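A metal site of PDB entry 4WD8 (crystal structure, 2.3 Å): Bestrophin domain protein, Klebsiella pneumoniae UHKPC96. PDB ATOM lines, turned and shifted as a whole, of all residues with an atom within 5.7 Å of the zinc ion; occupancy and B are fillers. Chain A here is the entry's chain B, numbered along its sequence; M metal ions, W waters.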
ATOM      1  N   ARG A 104     -24.771  12.566  28.394  1.00  0.00           N
ATOM      2  CA  ARG A 104     -24.173  11.574  27.507  1.00  0.00           C
ATOM      3  C   ARG A 104     -24.745  10.176  27.759  1.00  0.00           C
ATOM      4  O   ARG A 104     -25.015   9.431  26.810  1.00  0.00           O
ATOM      5  CB  ARG A 104     -22.640  11.587  27.626  1.00  0.00           C
ATOM      6  CG  ARG A 104     -21.971  12.790  26.931  1.00  0.00           C
ATOM      7  CD  ARG A 104     -20.512  13.005  27.341  1.00  0.00           C
ATOM      8  NE  ARG A 104     -19.831  13.978  26.469  1.00  0.00           N
ATOM      9  CZ  ARG A 104     -18.598  14.451  26.671  1.00  0.00           C
ATOM     10  NH1 ARG A 104     -18.075  15.330  25.814  1.00  0.00           N
ATOM     11  NH2 ARG A 104     -17.882  14.072  27.720  1.00  0.00           N
ATOM     12  N   PRO A 108     -27.434   9.842  24.597  1.00  0.00           N
ATOM     13  CA  PRO A 108     -26.131   9.747  23.933  1.00  0.00           C
ATOM     14  C   PRO A 108     -26.045  10.350  22.538  1.00  0.00           C
ATOM     15  O   PRO A 108     -24.958  10.733  22.122  1.00  0.00           O
ATOM     16  CB  PRO A 108     -25.882   8.234  23.854  1.00  0.00           C
ATOM     17  CG  PRO A 108     -27.234   7.614  23.972  1.00  0.00           C
ATOM     18  CD  PRO A 108     -27.989   8.521  24.902  1.00  0.00           C
ATOM     19  N   GLU A 110     -27.885  13.074  21.387  1.00  0.00           N
ATOM     20  CA  GLU A 110     -28.311  14.477  21.298  1.00  0.00           C
ATOM     21  C   GLU A 110     -27.122  15.447  21.352  1.00  0.00           C
ATOM     22  O   GLU A 110     -27.014  16.242  22.282  1.00  0.00           O
ATOM     23  CB  GLU A 110     -29.289  14.815  22.423  1.00  0.00           C
ATOM     24  CG  GLU A 110     -30.592  14.029  22.396  1.00  0.00           C
ATOM     25  CD  GLU A 110     -31.488  14.427  21.236  1.00  0.00           C
ATOM     26  OE1 GLU A 110     -31.421  15.592  20.788  1.00  0.00           O
ATOM     27  OE2 GLU A 110     -32.262  13.566  20.772  1.00  0.00           O
ATOM     28  N   HIS A 111     -26.261  15.385  20.352  1.00  0.00           N
ATOM     29  CA  HIS A 111     -25.014  16.146  20.377  1.00  0.00           C
ATOM     30  C   HIS A 111     -25.213  17.662  20.266  1.00  0.00           C
ATOM     31  O   HIS A 111     -24.432  18.424  20.844  1.00  0.00           O
ATOM     32  CB  HIS A 111     -24.015  15.651  19.324  1.00  0.00           C
ATOM     33  CG  HIS A 111     -23.700  14.189  19.430  1.00  0.00           C
ATOM     34  ND1 HIS A 111     -23.062  13.645  20.525  1.00  0.00           N
ATOM     35  CD2 HIS A 111     -23.885  13.172  18.557  1.00  0.00           C
ATOM     36  CE1 HIS A 111     -22.899  12.343  20.333  1.00  0.00           C
ATOM     37  NE2 HIS A 111     -23.385  12.033  19.139  1.00  0.00           N
ATOM     38  N   HIS A 114     -25.990  18.604  23.717  1.00  0.00           N
ATOM     39  CA  HIS A 114     -24.749  18.514  24.497  1.00  0.00           C
ATOM     40  C   HIS A 114     -23.939  19.792  24.352  1.00  0.00           C
ATOM     41  O   HIS A 114     -23.476  20.352  25.346  1.00  0.00           O
ATOM     42  CB  HIS A 114     -23.898  17.327  24.048  1.00  0.00           C
ATOM     43  CG  HIS A 114     -24.563  16.003  24.229  1.00  0.00           C
ATOM     44  ND1 HIS A 114     -24.140  14.866  23.565  1.00  0.00           N
ATOM     45  CD2 HIS A 114     -25.606  15.624  24.999  1.00  0.00           C
ATOM     46  CE1 HIS A 114     -24.900  13.850  23.930  1.00  0.00           C
ATOM     47  NE2 HIS A 114     -25.794  14.284  24.804  1.00  0.00           N
ATOM     48  N   GLY A 291     -15.437  17.513  22.291  1.00  0.00           N
ATOM     49  CA  GLY A 291     -16.708  17.182  22.892  1.00  0.00           C
ATOM     50  C   GLY A 291     -17.107  15.779  22.511  1.00  0.00           C
ATOM     51  O   GLY A 291     -18.245  15.371  22.738  1.00  0.00           O
ATOM     52  N   HIS A 293     -17.496  11.895  22.813  1.00  0.00           N
ATOM     53  CA  HIS A 293     -17.636  10.851  23.813  1.00  0.00           C
ATOM     54  C   HIS A 293     -17.965   9.501  23.179  1.00  0.00           C
ATOM     55  O   HIS A 293     -18.529   9.424  22.086  1.00  0.00           O
ATOM     56  CB  HIS A 293     -18.750  11.220  24.804  1.00  0.00           C
ATOM     57  CG  HIS A 293     -20.039  11.623  24.149  1.00  0.00           C
ATOM     58  ND1 HIS A 293     -21.151  10.807  24.128  1.00  0.00           N
ATOM     59  CD2 HIS A 293     -20.396  12.762  23.516  1.00  0.00           C
ATOM     60  CE1 HIS A 293     -22.139  11.427  23.507  1.00  0.00           C
ATOM     61  NE2 HIS A 293     -21.704  12.617  23.124  1.00  0.00           N
HETATM   62 ZN    ZN M   1     -22.507  14.378  22.410  1.00  0.00          ZN
HETATM   63  O   HOH W   1     -21.421  16.131  22.102  1.00  0.00           O
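ND1 of His 114 is bound to the zinc ion. A ring nitrogen (NE2) of His 293 binds the zinc ion. Water W1 is bound to the zinc ion. The zinc ion is bound by ND1 of His 111. The zinc ion has four donor atoms within binding distance.
Of the 7 residues printed, 3 come within 4 Å of the zinc ion.
A ring nitrogen (NE2) of His 114 sits close to the backbone carbonyl oxygen (O) of Glu 110 (3.4 Å).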
